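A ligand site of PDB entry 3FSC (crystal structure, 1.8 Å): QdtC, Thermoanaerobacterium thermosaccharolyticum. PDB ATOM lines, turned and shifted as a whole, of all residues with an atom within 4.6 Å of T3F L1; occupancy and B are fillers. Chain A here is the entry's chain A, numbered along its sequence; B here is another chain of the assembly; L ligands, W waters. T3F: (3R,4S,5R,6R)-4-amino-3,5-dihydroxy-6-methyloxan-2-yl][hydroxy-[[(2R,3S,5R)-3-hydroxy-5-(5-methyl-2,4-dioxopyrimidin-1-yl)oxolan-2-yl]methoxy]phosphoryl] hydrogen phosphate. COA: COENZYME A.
OE1 of Gln 122 of chain B lies within hydrogen-bond range of NH1 of Arg 104 of chain B (3.0 Å). The backbone carbonyl oxygen (O) of Glu 141 of chain B is in hydrogen-bond range of the side-chain amide nitrogen (ND2) of Asn 159 of chain B (2.9 Å). The side-chain hydroxyl of Ser 135 sits at hydrogen-bond distance from a ring nitrogen (ND1) of His 134 (3.5 Å). N of His 99 is in hydrogen-bond range of OG1 of Thr 117 (3.1 Å). The side-chain hydroxyl (OH) of Tyr 86 of chain B lies within hydrogen-bond range of a ring nitrogen (NE2) of His 99 (2.5 Å). OD2 of Asp 160 of chain B lies within hydrogen-bond range of OG of Ser 165 of chain B, 2.6 Å away. The guanidinium group (NH2) of Arg 104 of chain B sits close to a ring nitrogen (ND1) of His 123 of chain B, 3.3 Å away. The backbone NH (N) of Gly 116 sits at hydrogen-bond distance from the backbone carbonyl oxygen (O) of His 134, at 3.5 Å.
Water W3 lies within hydrogen-bond range of O1B of T3F L1 (2.5 Å), ND2 of Asn 132 (2.9 Å) and NZ of Lys 114 (3.5 Å). Water W11 lies within hydrogen-bond range of an oxygen (O4) of T3F L1 (2.7 Å), the backbone NH (N) of Val 58 of chain B (3.1 Å) and the guanidinium group (NH2) of Arg 80 (3.1 Å). Water W6 lies within hydrogen-bond range of OG1 of Thr 117 (2.7 Å), O2 of T3F L1 (2.7 Å) and NE2 of Gln 122 of chain B (3.3 Å). Water W10 lies within hydrogen-bond range of N3Q of T3F L1 (2.7 Å) and S1P of COA L2 (3.6 Å). Water W9 lies within hydrogen-bond range of an oxygen (O4) of T3F L1 (2.8 Å) and the backbone NH of Val 58 of chain B (3.1 Å). Water W7 bridges NH2 of Arg 104 of chain B (2.8 Å) and O2A of T3F L1 (2.8 Å).
A nitrogen (N3Q) of T3F L1 lies close to a sulfur (S1P) of COA L2 (3.2 Å).
Residues that only touch T3F L1: Gly 98 (3.7 Å), His 99 (3.2 Å), Gly 116 (3.2 Å), Trp 150 (3.8 Å), Phe 152 (3.6 Å), Gln 122 of chain B (3.7 Å), Pro 164 of chain B (3.4 Å), Ser 165 of chain B (3.99 Å) and Leu 168 of chain B (3.3 Å). Within 4 Å of T3F L1: Arg 80, Gly 98, His 99, Lys 114, Gly 116, Thr 117, His 134, Ser 135, Trp 150, Phe 152, Arg 245, Tyr 86 of chain B, Arg 104 of chain B, Gln 122 of chain B, Glu 141 of chain B, Asn 159 of chain B, Asp 160 of chain B, Pro 164 of chain B, Ser 165 of chain B and Leu 168 of chain B.
N of Thr 117 lies within hydrogen-bond range of O3' of T3F L1, at 3.0 Å. O3' of T3F L1 sits at hydrogen-bond distance from OG of Ser 135, 2.7 Å away. The backbone NH (N) of Asn 159 of chain B lies close to a sulfur (S1P) of COA L2 (3.3 Å). The side-chain carboxylate (OE2) of Glu 141 of chain B is in salt-bridge range of a nitrogen (N3Q) of T3F L1 (3.8 Å). S1P of COA L2 lies close to N of Asp 160 of chain B. OD1 of Asp 160 of chain B sits at hydrogen-bond distance from O4Q of T3F L1 (2.7 Å). OG1 of Thr 117 lies within hydrogen-bond range of O2 of T3F L1. A nitrogen (N3Q) of T3F L1 lies within hydrogen-bond range of the side-chain amide oxygen (OD1) of Asn 159 of chain B. The side-chain amide oxygen (OD1) of Asn 159 of chain B sits close to a sulfur (S1P) of COA L2, 3.3 Å away. O of Asp 160 of chain B sits at hydrogen-bond distance from N4P of COA L2 (3.0 Å). The guanidinium group (NH1) of Arg 104 of chain B is in salt-bridge range of an oxygen (O2A) of T3F L1, 2.8 Å away. The guanidinium group (NH1) of Arg 245 lies within salt-bridge range of an oxygen (O2B) of T3F L1. NE2 of His 134 is in hydrogen-bond range of O2Q of T3F L1, 3.4 Å away. The side-chain hydroxyl (OH) of Tyr 86 of chain B lies within hydrogen-bond range of a nitrogen (N3) of T3F L1 (2.7 Å). NH2 of Arg 80 lies within hydrogen-bond range of O4 of T3F L1 (3.3 Å). NZ of Lys 114 lies within salt-bridge range of O1A of T3F L1 (2.8 Å).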
ATOM      1  N   ARG A  80     -12.040 -37.672  14.728  1.00  0.00           N
ATOM      2  CA  ARG A  80     -12.051 -36.897  15.948  1.00  0.00           C
ATOM      3  C   ARG A  80     -12.660 -37.579  17.190  1.00  0.00           C
ATOM      4  O   ARG A  80     -13.069 -38.751  17.180  1.00  0.00           O
ATOM      5  CB  ARG A  80     -12.292 -35.387  15.749  1.00  0.00           C
ATOM      6  CG  ARG A  80     -11.210 -34.729  14.867  1.00  0.00           C
ATOM      7  CD  ARG A  80     -11.345 -33.179  14.881  1.00  0.00           C
ATOM      8  NE  ARG A  80     -10.348 -32.447  14.084  1.00  0.00           N
ATOM      9  CZ  ARG A  80     -10.314 -32.410  12.745  1.00  0.00           C
ATOM     10  NH1 ARG A  80     -11.211 -33.079  11.999  1.00  0.00           N
ATOM     11  NH2 ARG A  80      -9.354 -31.698  12.160  1.00  0.00           N
ATOM     12  N   GLY A  98     -15.555 -34.839  12.367  1.00  0.00           N
ATOM     13  CA  GLY A  98     -15.626 -33.833  13.411  1.00  0.00           C
ATOM     14  C   GLY A  98     -15.895 -34.648  14.693  1.00  0.00           C
ATOM     15  O   GLY A  98     -15.680 -35.860  14.795  1.00  0.00           O
ATOM     16  N   HIS A  99     -16.391 -33.975  15.723  1.00  0.00           N
ATOM     17  CA  HIS A  99     -16.639 -34.619  17.010  1.00  0.00           C
ATOM     18  C   HIS A  99     -17.925 -35.350  17.240  1.00  0.00           C
ATOM     19  O   HIS A  99     -18.985 -34.875  16.786  1.00  0.00           O
ATOM     20  CB  HIS A  99     -16.443 -33.553  18.153  1.00  0.00           C
ATOM     21  CG  HIS A  99     -15.083 -32.935  18.073  1.00  0.00           C
ATOM     22  ND1 HIS A  99     -14.005 -33.385  18.812  1.00  0.00           N
ATOM     23  CD2 HIS A  99     -14.620 -31.940  17.266  1.00  0.00           C
ATOM     24  CE1 HIS A  99     -12.935 -32.703  18.451  1.00  0.00           C
ATOM     25  NE2 HIS A  99     -13.272 -31.800  17.528  1.00  0.00           N
ATOM     26  N   LYS A 114     -15.516 -36.503   4.255  1.00  0.00           N
ATOM     27  CA  LYS A 114     -15.485 -35.747   5.499  1.00  0.00           C
ATOM     28  C   LYS A 114     -16.864 -35.736   6.142  1.00  0.00           C
ATOM     29  O   LYS A 114     -17.830 -35.452   5.456  1.00  0.00           O
ATOM     30  CB  LYS A 114     -15.096 -34.320   5.202  1.00  0.00           C
ATOM     31  CG  LYS A 114     -13.630 -34.174   5.001  1.00  0.00           C
ATOM     32  CD  LYS A 114     -13.368 -32.718   4.549  1.00  0.00           C
ATOM     33  CE  LYS A 114     -13.247 -31.738   5.710  1.00  0.00           C
ATOM     34  NZ  LYS A 114     -13.388 -30.318   5.212  1.00  0.00           N
ATOM     35  N   GLY A 116     -18.906 -34.275   9.451  1.00  0.00           N
ATOM     36  CA  GLY A 116     -18.792 -33.348  10.564  1.00  0.00           C
ATOM     37  C   GLY A 116     -19.461 -33.669  11.893  1.00  0.00           C
ATOM     38  O   GLY A 116     -20.271 -34.598  12.063  1.00  0.00           O
ATOM     39  N   THR A 117     -19.110 -32.816  12.835  1.00  0.00           N
ATOM     40  CA  THR A 117     -19.558 -32.887  14.225  1.00  0.00           C
ATOM     41  C   THR A 117     -21.050 -33.190  14.371  1.00  0.00           C
ATOM     42  O   THR A 117     -21.875 -32.520  13.751  1.00  0.00           O
ATOM     43  CB  THR A 117     -19.166 -31.589  14.954  1.00  0.00           C
ATOM     44  OG1 THR A 117     -17.745 -31.370  14.891  1.00  0.00           O
ATOM     45  CG2 THR A 117     -19.713 -31.599  16.400  1.00  0.00           C
ATOM     46  N   ASN A 132     -18.639 -34.422   1.274  1.00  0.00           N
ATOM     47  CA  ASN A 132     -18.494 -33.534   2.440  1.00  0.00           C
ATOM     48  C   ASN A 132     -19.824 -33.442   3.190  1.00  0.00           C
ATOM     49  O   ASN A 132     -20.777 -32.872   2.656  1.00  0.00           O
ATOM     50  CB  ASN A 132     -18.098 -32.112   1.981  1.00  0.00           C
ATOM     51  CG  ASN A 132     -16.659 -32.058   1.637  1.00  0.00           C
ATOM     52  OD1 ASN A 132     -16.244 -32.078   0.469  1.00  0.00           O
ATOM     53  ND2 ASN A 132     -15.861 -32.129   2.691  1.00  0.00           N
ATOM     54  N   HIS A 134     -21.356 -31.977   6.503  1.00  0.00           N
ATOM     55  CA  HIS A 134     -20.997 -31.000   7.546  1.00  0.00           C
ATOM     56  C   HIS A 134     -21.610 -31.325   8.912  1.00  0.00           C
ATOM     57  O   HIS A 134     -21.883 -32.491   9.209  1.00  0.00           O
ATOM     58  CB  HIS A 134     -21.167 -29.540   6.944  1.00  0.00           C
ATOM     59  CG  HIS A 134     -20.291 -28.474   7.543  1.00  0.00           C
ATOM     60  ND1 HIS A 134     -20.337 -28.118   8.891  1.00  0.00           N
ATOM     61  CD2 HIS A 134     -19.397 -27.629   6.964  1.00  0.00           C
ATOM     62  CE1 HIS A 134     -19.483 -27.112   9.100  1.00  0.00           C
ATOM     63  NE2 HIS A 134     -18.900 -26.803   7.958  1.00  0.00           N
ATOM     64  N   SER A 135     -21.796 -30.347   9.777  1.00  0.00           N
ATOM     65  CA  SER A 135     -22.335 -30.608  11.107  1.00  0.00           C
ATOM     66  C   SER A 135     -23.803 -31.059  11.215  1.00  0.00           C
ATOM     67  O   SER A 135     -24.696 -30.488  10.597  1.00  0.00           O
ATOM     68  CB  SER A 135     -22.168 -29.397  12.074  1.00  0.00           C
ATOM     69  OG  SER A 135     -20.805 -29.001  12.209  1.00  0.00           O
ATOM     70  N   TRP A 150     -22.259 -32.410  -1.423  1.00  0.00           N
ATOM     71  CA  TRP A 150     -22.079 -31.648  -0.189  1.00  0.00           C
ATOM     72  C   TRP A 150     -23.397 -31.606   0.578  1.00  0.00           C
ATOM     73  O   TRP A 150     -24.436 -31.256  -0.011  1.00  0.00           O
ATOM     74  CB  TRP A 150     -21.857 -30.173  -0.498  1.00  0.00           C
ATOM     75  CG  TRP A 150     -20.507 -29.967  -1.096  1.00  0.00           C
ATOM     76  CD1 TRP A 150     -20.138 -30.186  -2.398  1.00  0.00           C
ATOM     77  CD2 TRP A 150     -19.365 -29.433  -0.424  1.00  0.00           C
ATOM     78  NE1 TRP A 150     -18.812 -29.810  -2.572  1.00  0.00           N
ATOM     79  CE2 TRP A 150     -18.311 -29.357  -1.378  1.00  0.00           C
ATOM     80  CE3 TRP A 150     -19.118 -29.043   0.890  1.00  0.00           C
ATOM     81  CZ2 TRP A 150     -17.030 -28.902  -1.055  1.00  0.00           C
ATOM     82  CZ3 TRP A 150     -17.837 -28.563   1.215  1.00  0.00           C
ATOM     83  CH2 TRP A 150     -16.818 -28.506   0.252  1.00  0.00           C
ATOM     84  N   PHE A 152     -24.782 -29.753   3.802  1.00  0.00           N
ATOM     85  CA  PHE A 152     -24.565 -28.682   4.772  1.00  0.00           C
ATOM     86  C   PHE A 152     -25.210 -28.912   6.145  1.00  0.00           C
ATOM     87  O   PHE A 152     -26.041 -29.827   6.314  1.00  0.00           O
ATOM     88  CB  PHE A 152     -24.715 -27.322   4.070  1.00  0.00           C
ATOM     89  CG  PHE A 152     -23.535 -27.037   3.218  1.00  0.00           C
ATOM     90  CD1 PHE A 152     -22.315 -26.726   3.837  1.00  0.00           C
ATOM     91  CD2 PHE A 152     -23.619 -27.150   1.831  1.00  0.00           C
ATOM     92  CE1 PHE A 152     -21.173 -26.421   3.058  1.00  0.00           C
ATOM     93  CE2 PHE A 152     -22.500 -26.897   1.039  1.00  0.00           C
ATOM     94  CZ  PHE A 152     -21.262 -26.544   1.618  1.00  0.00           C
ATOM     95  N   PHE A 243     -14.419 -23.973  -7.408  1.00  0.00           N
ATOM     96  CA  PHE A 243     -14.000 -24.347  -6.059  1.00  0.00           C
ATOM     97  C   PHE A 243     -13.141 -25.590  -6.128  1.00  0.00           C
ATOM     98  O   PHE A 243     -13.526 -26.581  -6.734  1.00  0.00           O
ATOM     99  CB  PHE A 243     -15.242 -24.562  -5.150  1.00  0.00           C
ATOM    100  CG  PHE A 243     -14.889 -24.914  -3.727  1.00  0.00           C
ATOM    101  CD1 PHE A 243     -14.802 -23.913  -2.746  1.00  0.00           C
ATOM    102  CD2 PHE A 243     -14.596 -26.247  -3.383  1.00  0.00           C
ATOM    103  CE1 PHE A 243     -14.407 -24.235  -1.449  1.00  0.00           C
ATOM    104  CE2 PHE A 243     -14.238 -26.589  -2.075  1.00  0.00           C
ATOM    105  CZ  PHE A 243     -14.128 -25.559  -1.116  1.00  0.00           C
ATOM    106  N   ARG A 245     -10.656 -26.456  -3.295  1.00  0.00           N
ATOM    107  CA  ARG A 245     -10.002 -26.722  -2.043  1.00  0.00           C
ATOM    108  C   ARG A 245     -10.346 -28.149  -1.646  1.00  0.00           C
ATOM    109  O   ARG A 245     -11.518 -28.501  -1.558  1.00  0.00           O
ATOM    110  CB  ARG A 245     -10.567 -25.807  -0.969  1.00  0.00           C
ATOM    111  CG  ARG A 245     -10.094 -26.209   0.416  1.00  0.00           C
ATOM    112  CD  ARG A 245     -10.252 -25.008   1.334  1.00  0.00           C
ATOM    113  NE  ARG A 245     -11.597 -24.412   1.409  1.00  0.00           N
ATOM    114  CZ  ARG A 245     -12.582 -24.874   2.178  1.00  0.00           C
ATOM    115  NH1 ARG A 245     -12.401 -25.931   2.940  1.00  0.00           N
ATOM    116  NH2 ARG A 245     -13.741 -24.269   2.202  1.00  0.00           N
ATOM    117  N   VAL B  58      -5.973 -28.067  13.680  1.00  0.00           N
ATOM    118  CA  VAL B  58      -5.595 -28.817  12.505  1.00  0.00           C
ATOM    119  C   VAL B  58      -4.117 -29.039  12.329  1.00  0.00           C
ATOM    120  O   VAL B  58      -3.677 -30.109  11.917  1.00  0.00           O
ATOM    121  CB  VAL B  58      -6.264 -28.254  11.207  1.00  0.00           C
ATOM    122  CG1 VAL B  58      -5.229 -27.542  10.336  1.00  0.00           C
ATOM    123  CG2 VAL B  58      -6.897 -29.391  10.466  1.00  0.00           C
ATOM    124  N   TYR B  86     -11.705 -25.949  21.869  1.00  0.00           N
ATOM    125  CA  TYR B  86     -10.436 -25.752  21.152  1.00  0.00           C
ATOM    126  C   TYR B  86      -9.501 -24.688  21.718  1.00  0.00           C
ATOM    127  O   TYR B  86      -9.908 -23.834  22.502  1.00  0.00           O
ATOM    128  CB  TYR B  86     -10.666 -25.415  19.665  1.00  0.00           C
ATOM    129  CG  TYR B  86     -11.022 -26.638  18.818  1.00  0.00           C
ATOM    130  CD1 TYR B  86     -10.315 -26.928  17.672  1.00  0.00           C
ATOM    131  CD2 TYR B  86     -12.044 -27.518  19.194  1.00  0.00           C
ATOM    132  CE1 TYR B  86     -10.612 -28.000  16.907  1.00  0.00           C
ATOM    133  CE2 TYR B  86     -12.342 -28.639  18.410  1.00  0.00           C
ATOM    134  CZ  TYR B  86     -11.619 -28.872  17.272  1.00  0.00           C
ATOM    135  OH  TYR B  86     -11.865 -29.982  16.455  1.00  0.00           O
ATOM    136  N   ARG B 104     -15.110 -24.334  18.715  1.00  0.00           N
ATOM    137  CA  ARG B 104     -13.865 -24.255  17.954  1.00  0.00           C
ATOM    138  C   ARG B 104     -12.842 -23.168  18.288  1.00  0.00           C
ATOM    139  O   ARG B 104     -12.968 -22.365  19.238  1.00  0.00           O
ATOM    140  CB  ARG B 104     -14.043 -24.553  16.448  1.00  0.00           C
ATOM    141  CG  ARG B 104     -13.969 -26.038  16.081  1.00  0.00           C
ATOM    142  CD  ARG B 104     -14.280 -26.278  14.600  1.00  0.00           C
ATOM    143  NE  ARG B 104     -13.093 -25.845  13.867  1.00  0.00           N
ATOM    144  CZ  ARG B 104     -12.959 -25.956  12.541  1.00  0.00           C
ATOM    145  NH1 ARG B 104     -13.936 -26.499  11.811  1.00  0.00           N
ATOM    146  NH2 ARG B 104     -11.833 -25.516  11.950  1.00  0.00           N
ATOM    147  N   GLN B 122     -18.519 -22.811  15.767  1.00  0.00           N
ATOM    148  CA  GLN B 122     -17.408 -23.025  14.849  1.00  0.00           C
ATOM    149  C   GLN B 122     -16.283 -22.044  15.190  1.00  0.00           C
ATOM    150  O   GLN B 122     -16.393 -21.321  16.197  1.00  0.00           O
ATOM    151  CB  GLN B 122     -17.921 -22.964  13.418  1.00  0.00           C
ATOM    152  CG  GLN B 122     -18.690 -24.261  13.079  1.00  0.00           C
ATOM    153  CD  GLN B 122     -17.771 -25.487  13.087  1.00  0.00           C
ATOM    154  OE1 GLN B 122     -16.696 -25.465  12.456  1.00  0.00           O
ATOM    155  NE2 GLN B 122     -18.209 -26.565  13.737  1.00  0.00           N
ATOM    156  N   HIS B 123     -15.256 -21.999  14.360  1.00  0.00           N
ATOM    157  CA  HIS B 123     -14.111 -21.127  14.596  1.00  0.00           C
ATOM    158  C   HIS B 123     -14.390 -19.684  14.203  1.00  0.00           C
ATOM    159  O   HIS B 123     -15.339 -19.421  13.412  1.00  0.00           O
ATOM    160  CB  HIS B 123     -12.923 -21.772  13.820  1.00  0.00           C
ATOM    161  CG  HIS B 123     -13.130 -21.869  12.347  1.00  0.00           C
ATOM    162  ND1 HIS B 123     -13.855 -22.887  11.733  1.00  0.00           N
ATOM    163  CD2 HIS B 123     -12.738 -21.047  11.354  1.00  0.00           C
ATOM    164  CE1 HIS B 123     -13.872 -22.678  10.430  1.00  0.00           C
ATOM    165  NE2 HIS B 123     -13.193 -21.579  10.167  1.00  0.00           N
ATOM    166  N   GLU B 141     -18.696 -20.244  11.336  1.00  0.00           N
ATOM    167  CA  GLU B 141     -17.629 -19.245  11.369  1.00  0.00           C
ATOM    168  C   GLU B 141     -18.040 -17.894  10.817  1.00  0.00           C
ATOM    169  O   GLU B 141     -18.847 -17.780   9.856  1.00  0.00           O
ATOM    170  CB  GLU B 141     -16.367 -19.747  10.634  1.00  0.00           C
ATOM    171  CG  GLU B 141     -16.502 -20.023   9.148  1.00  0.00           C
ATOM    172  CD  GLU B 141     -17.006 -21.428   8.799  1.00  0.00           C
ATOM    173  OE1 GLU B 141     -17.731 -22.137   9.544  1.00  0.00           O
ATOM    174  OE2 GLU B 141     -16.667 -21.855   7.676  1.00  0.00           O
ATOM    175  N   ASN B 159     -22.943 -19.291   6.438  1.00  0.00           N
ATOM    176  CA  ASN B 159     -21.975 -18.288   5.946  1.00  0.00           C
ATOM    177  C   ASN B 159     -21.506 -18.437   4.500  1.00  0.00           C
ATOM    178  O   ASN B 159     -20.810 -17.553   3.972  1.00  0.00           O
ATOM    179  CB  ASN B 159     -20.737 -18.286   6.847  1.00  0.00           C
ATOM    180  CG  ASN B 159     -20.089 -19.656   6.951  1.00  0.00           C
ATOM    181  OD1 ASN B 159     -20.011 -20.427   5.977  1.00  0.00           O
ATOM    182  ND2 ASN B 159     -19.656 -19.998   8.175  1.00  0.00           N
ATOM    183  N   ASP B 160     -21.843 -19.547   3.835  1.00  0.00           N
ATOM    184  CA  ASP B 160     -21.393 -19.636   2.424  1.00  0.00           C
ATOM    185  C   ASP B 160     -22.589 -19.303   1.510  1.00  0.00           C
ATOM    186  O   ASP B 160     -23.509 -20.096   1.367  1.00  0.00           O
ATOM    187  CB  ASP B 160     -20.854 -21.045   2.182  1.00  0.00           C
ATOM    188  CG  ASP B 160     -20.295 -21.204   0.814  1.00  0.00           C
ATOM    189  OD1 ASP B 160     -19.456 -22.081   0.706  1.00  0.00           O
ATOM    190  OD2 ASP B 160     -20.645 -20.452  -0.107  1.00  0.00           O
ATOM    191  N   PRO B 164     -20.353 -24.781  -2.620  1.00  0.00           N
ATOM    192  CA  PRO B 164     -19.208 -24.389  -1.824  1.00  0.00           C
ATOM    193  C   PRO B 164     -18.549 -23.252  -2.590  1.00  0.00           C
ATOM    194  O   PRO B 164     -18.528 -23.270  -3.838  1.00  0.00           O
ATOM    195  CB  PRO B 164     -18.323 -25.642  -1.863  1.00  0.00           C
ATOM    196  CG  PRO B 164     -18.635 -26.306  -3.227  1.00  0.00           C
ATOM    197  CD  PRO B 164     -20.148 -26.037  -3.381  1.00  0.00           C
ATOM    198  N   SER B 165     -18.057 -22.260  -1.853  1.00  0.00           N
ATOM    199  CA  SER B 165     -17.364 -21.089  -2.380  1.00  0.00           C
ATOM    200  C   SER B 165     -16.287 -20.662  -1.430  1.00  0.00           C
ATOM    201  O   SER B 165     -16.210 -21.119  -0.282  1.00  0.00           O
ATOM    202  CB  SER B 165     -18.190 -19.893  -2.819  1.00  0.00           C
ATOM    203  OG  SER B 165     -19.058 -19.352  -1.808  1.00  0.00           O
ATOM    204  N   LEU B 168     -16.667 -16.190   2.366  1.00  0.00           N
ATOM    205  CA  LEU B 168     -17.773 -16.325   3.317  1.00  0.00           C
ATOM    206  C   LEU B 168     -18.253 -15.013   3.906  1.00  0.00           C
ATOM    207  O   LEU B 168     -17.502 -14.053   4.012  1.00  0.00           O
ATOM    208  CB  LEU B 168     -17.384 -17.281   4.460  1.00  0.00           C
ATOM    209  CG  LEU B 168     -16.839 -18.616   4.000  1.00  0.00           C
ATOM    210  CD1 LEU B 168     -16.290 -19.424   5.177  1.00  0.00           C
ATOM    211  CD2 LEU B 168     -17.803 -19.351   3.093  1.00  0.00           C
HETATM  212  O2B T3F L   1     -13.931 -26.857   4.977  1.00  0.00           O
HETATM  213  PB  T3F L   1     -15.384 -27.182   5.568  1.00  0.00           P
HETATM  214  O1B T3F L   1     -15.863 -28.526   5.170  1.00  0.00           O
HETATM  215  O3B T3F L   1     -16.541 -26.190   5.041  1.00  0.00           O
HETATM  216  C1Q T3F L   1     -16.182 -24.804   4.765  1.00  0.00           C
HETATM  217  O5Q T3F L   1     -16.163 -24.687   3.352  1.00  0.00           O
HETATM  218  C5Q T3F L   1     -17.449 -24.986   2.801  1.00  0.00           C
HETATM  219  C6Q T3F L   1     -17.302 -24.769   1.286  1.00  0.00           C
HETATM  220  C2Q T3F L   1     -17.124 -23.790   5.444  1.00  0.00           C
HETATM  221  O2Q T3F L   1     -17.123 -24.120   6.841  1.00  0.00           O
HETATM  222  C3Q T3F L   1     -18.540 -23.997   4.872  1.00  0.00           C
HETATM  223  N3Q T3F L   1     -19.491 -22.980   5.429  1.00  0.00           N
HETATM  224  C4Q T3F L   1     -18.491 -23.976   3.320  1.00  0.00           C
HETATM  225  O4Q T3F L   1     -18.052 -22.667   2.895  1.00  0.00           O
HETATM  226  O3A T3F L   1     -15.424 -26.927   7.168  1.00  0.00           O
HETATM  227  PA  T3F L   1     -14.451 -27.768   8.165  1.00  0.00           P
HETATM  228  O1A T3F L   1     -13.436 -28.695   7.537  1.00  0.00           O
HETATM  229  O2A T3F L   1     -13.706 -26.604   8.986  1.00  0.00           O
HETATM  230  O5' T3F L   1     -15.463 -28.469   9.205  1.00  0.00           O
HETATM  231  C5' T3F L   1     -16.144 -29.575   8.624  1.00  0.00           C
HETATM  232  C4' T3F L   1     -16.713 -30.403   9.778  1.00  0.00           C
HETATM  233  O4' T3F L   1     -15.645 -31.034  10.575  1.00  0.00           O
HETATM  234  C3' T3F L   1     -17.509 -29.489  10.772  1.00  0.00           C
HETATM  235  O3' T3F L   1     -18.522 -30.254  11.412  1.00  0.00           O
HETATM  236  C2' T3F L   1     -16.456 -29.170  11.852  1.00  0.00           C
HETATM  237  C1' T3F L   1     -15.599 -30.502  11.902  1.00  0.00           C
HETATM  238  N1  T3F L   1     -14.206 -30.083  12.224  1.00  0.00           N
HETATM  239  C2  T3F L   1     -13.790 -30.051  13.531  1.00  0.00           C
HETATM  240  O2  T3F L   1     -14.542 -30.392  14.451  1.00  0.00           O
HETATM  241  N3  T3F L   1     -12.539 -29.627  13.846  1.00  0.00           N
HETATM  242  C6  T3F L   1     -13.321 -29.697  11.223  1.00  0.00           C
HETATM  243  C5  T3F L   1     -12.055 -29.272  11.505  1.00  0.00           C
HETATM  244  C5M T3F L   1     -11.121 -28.852  10.374  1.00  0.00           C
HETATM  245  C4  T3F L   1     -11.648 -29.214  12.893  1.00  0.00           C
HETATM  246  O4  T3F L   1     -10.520 -28.822  13.255  1.00  0.00           O
HETATM  247  N1A COA L   2     -35.680 -20.427   0.753  1.00  0.00           N
HETATM  248  C2A COA L   2     -36.755 -19.729   0.367  1.00  0.00           C
HETATM  249  N3A COA L   2     -36.686 -18.653  -0.426  1.00  0.00           N
HETATM  250  C4A COA L   2     -35.463 -18.266  -0.846  1.00  0.00           C
HETATM  251  C5A COA L   2     -34.283 -18.989  -0.462  1.00  0.00           C
HETATM  252  C6A COA L   2     -34.432 -20.099   0.361  1.00  0.00           C
HETATM  253  N6A COA L   2     -33.295 -20.837   0.732  1.00  0.00           N
HETATM  254  N7A COA L   2     -33.214 -18.380  -1.045  1.00  0.00           N
HETATM  255  C8A COA L   2     -33.647 -17.344  -1.726  1.00  0.00           C
HETATM  256  N9A COA L   2     -35.006 -17.234  -1.635  1.00  0.00           N
HETATM  257  C1B COA L   2     -35.853 -16.200  -2.240  1.00  0.00           C
HETATM  258  C2B COA L   2     -35.356 -14.750  -1.850  1.00  0.00           C
HETATM  259  O2B COA L   2     -35.918 -14.273  -0.608  1.00  0.00           O
HETATM  260  C3B COA L   2     -35.955 -13.960  -3.053  1.00  0.00           C
HETATM  261  O3B COA L   2     -37.379 -13.909  -2.815  1.00  0.00           O
HETATM  262  P3B COA L   2     -38.155 -12.487  -3.039  1.00  0.00           P
HETATM  263  O7A COA L   2     -37.226 -11.543  -3.684  1.00  0.00           O
HETATM  264  O8A COA L   2     -39.479 -12.685  -3.942  1.00  0.00           O
HETATM  265  O9A COA L   2     -38.641 -12.018  -1.568  1.00  0.00           O
HETATM  266  C4B COA L   2     -35.652 -14.956  -4.214  1.00  0.00           C
HETATM  267  O4B COA L   2     -35.736 -16.303  -3.677  1.00  0.00           O
HETATM  268  C5B COA L   2     -34.217 -14.865  -4.760  1.00  0.00           C
HETATM  269  O5B COA L   2     -33.461 -14.391  -3.683  1.00  0.00           O
HETATM  270  P1A COA L   2     -31.949 -14.563  -4.127  1.00  0.00           P
HETATM  271  O1A COA L   2     -31.201 -13.782  -3.095  1.00  0.00           O
HETATM  272  O2A COA L   2     -31.661 -13.986  -5.593  1.00  0.00           O
HETATM  273  O3A COA L   2     -31.587 -16.114  -4.143  1.00  0.00           O
HETATM  274  P2A COA L   2     -30.125 -16.275  -3.497  1.00  0.00           P
HETATM  275  O4A COA L   2     -29.152 -16.289  -4.631  1.00  0.00           O
HETATM  276  O5A COA L   2     -29.813 -15.147  -2.371  1.00  0.00           O
HETATM  277  O6A COA L   2     -30.103 -17.614  -2.603  1.00  0.00           O
HETATM  278  CBP COA L   2     -29.464 -19.851  -2.624  1.00  0.00           C
HETATM  279  CCP COA L   2     -30.239 -18.778  -3.400  1.00  0.00           C
HETATM  280  CDP COA L   2     -27.975 -19.676  -3.015  1.00  0.00           C
HETATM  281  CEP COA L   2     -29.978 -21.237  -3.066  1.00  0.00           C
HETATM  282  CAP COA L   2     -29.681 -19.648  -1.085  1.00  0.00           C
HETATM  283  OAP COA L   2     -31.055 -19.835  -0.747  1.00  0.00           O
HETATM  284  C9P COA L   2     -28.868 -20.628  -0.300  1.00  0.00           C
HETATM  285  O9P COA L   2     -29.277 -21.746  -0.066  1.00  0.00           O
HETATM  286  N8P COA L   2     -27.655 -20.313   0.162  1.00  0.00           N
HETATM  287  C7P COA L   2     -26.969 -21.376   0.876  1.00  0.00           C
HETATM  288  C6P COA L   2     -26.848 -21.075   2.379  1.00  0.00           C
HETATM  289  C5P COA L   2     -26.148 -22.299   2.940  1.00  0.00           C
HETATM  290  O5P COA L   2     -26.793 -23.197   3.435  1.00  0.00           O
HETATM  291  N4P COA L   2     -24.809 -22.371   2.849  1.00  0.00           N
HETATM  292  C3P COA L   2     -24.106 -23.552   3.352  1.00  0.00           C
HETATM  293  C2P COA L   2     -23.919 -23.561   4.868  1.00  0.00           C
HETATM  294  S1P COA L   2     -22.634 -22.369   5.308  1.00  0.00           S
HETATM  295  O   HOH W   1     -14.854 -33.203   8.956  1.00  0.00           O
HETATM  296  O   HOH W   2     -17.070 -24.849   9.710  1.00  0.00           O
HETATM  297  O   HOH W   3     -16.825 -30.843   5.081  1.00  0.00           O
HETATM  298  O   HOH W   4     -14.572 -24.366   8.321  1.00  0.00           O
HETATM  299  O   HOH W   5     -15.375 -21.868   2.134  1.00  0.00           O
HETATM  300  O   HOH W   6     -16.658 -28.949  15.357  1.00  0.00           O
HETATM  301  O   HOH W   7     -11.229 -25.217   9.213  1.00  0.00           O
HETATM  302  O   HOH W   8     -17.256 -32.407   7.321  1.00  0.00           O
HETATM  303  O   HOH W   9      -8.768 -26.715  13.932  1.00  0.00           O
HETATM  304  O   HOH W  10     -20.516 -23.619   7.892  1.00  0.00           O
HETATM  305  O   HOH W  11      -8.362 -29.873  14.516  1.00  0.00           O
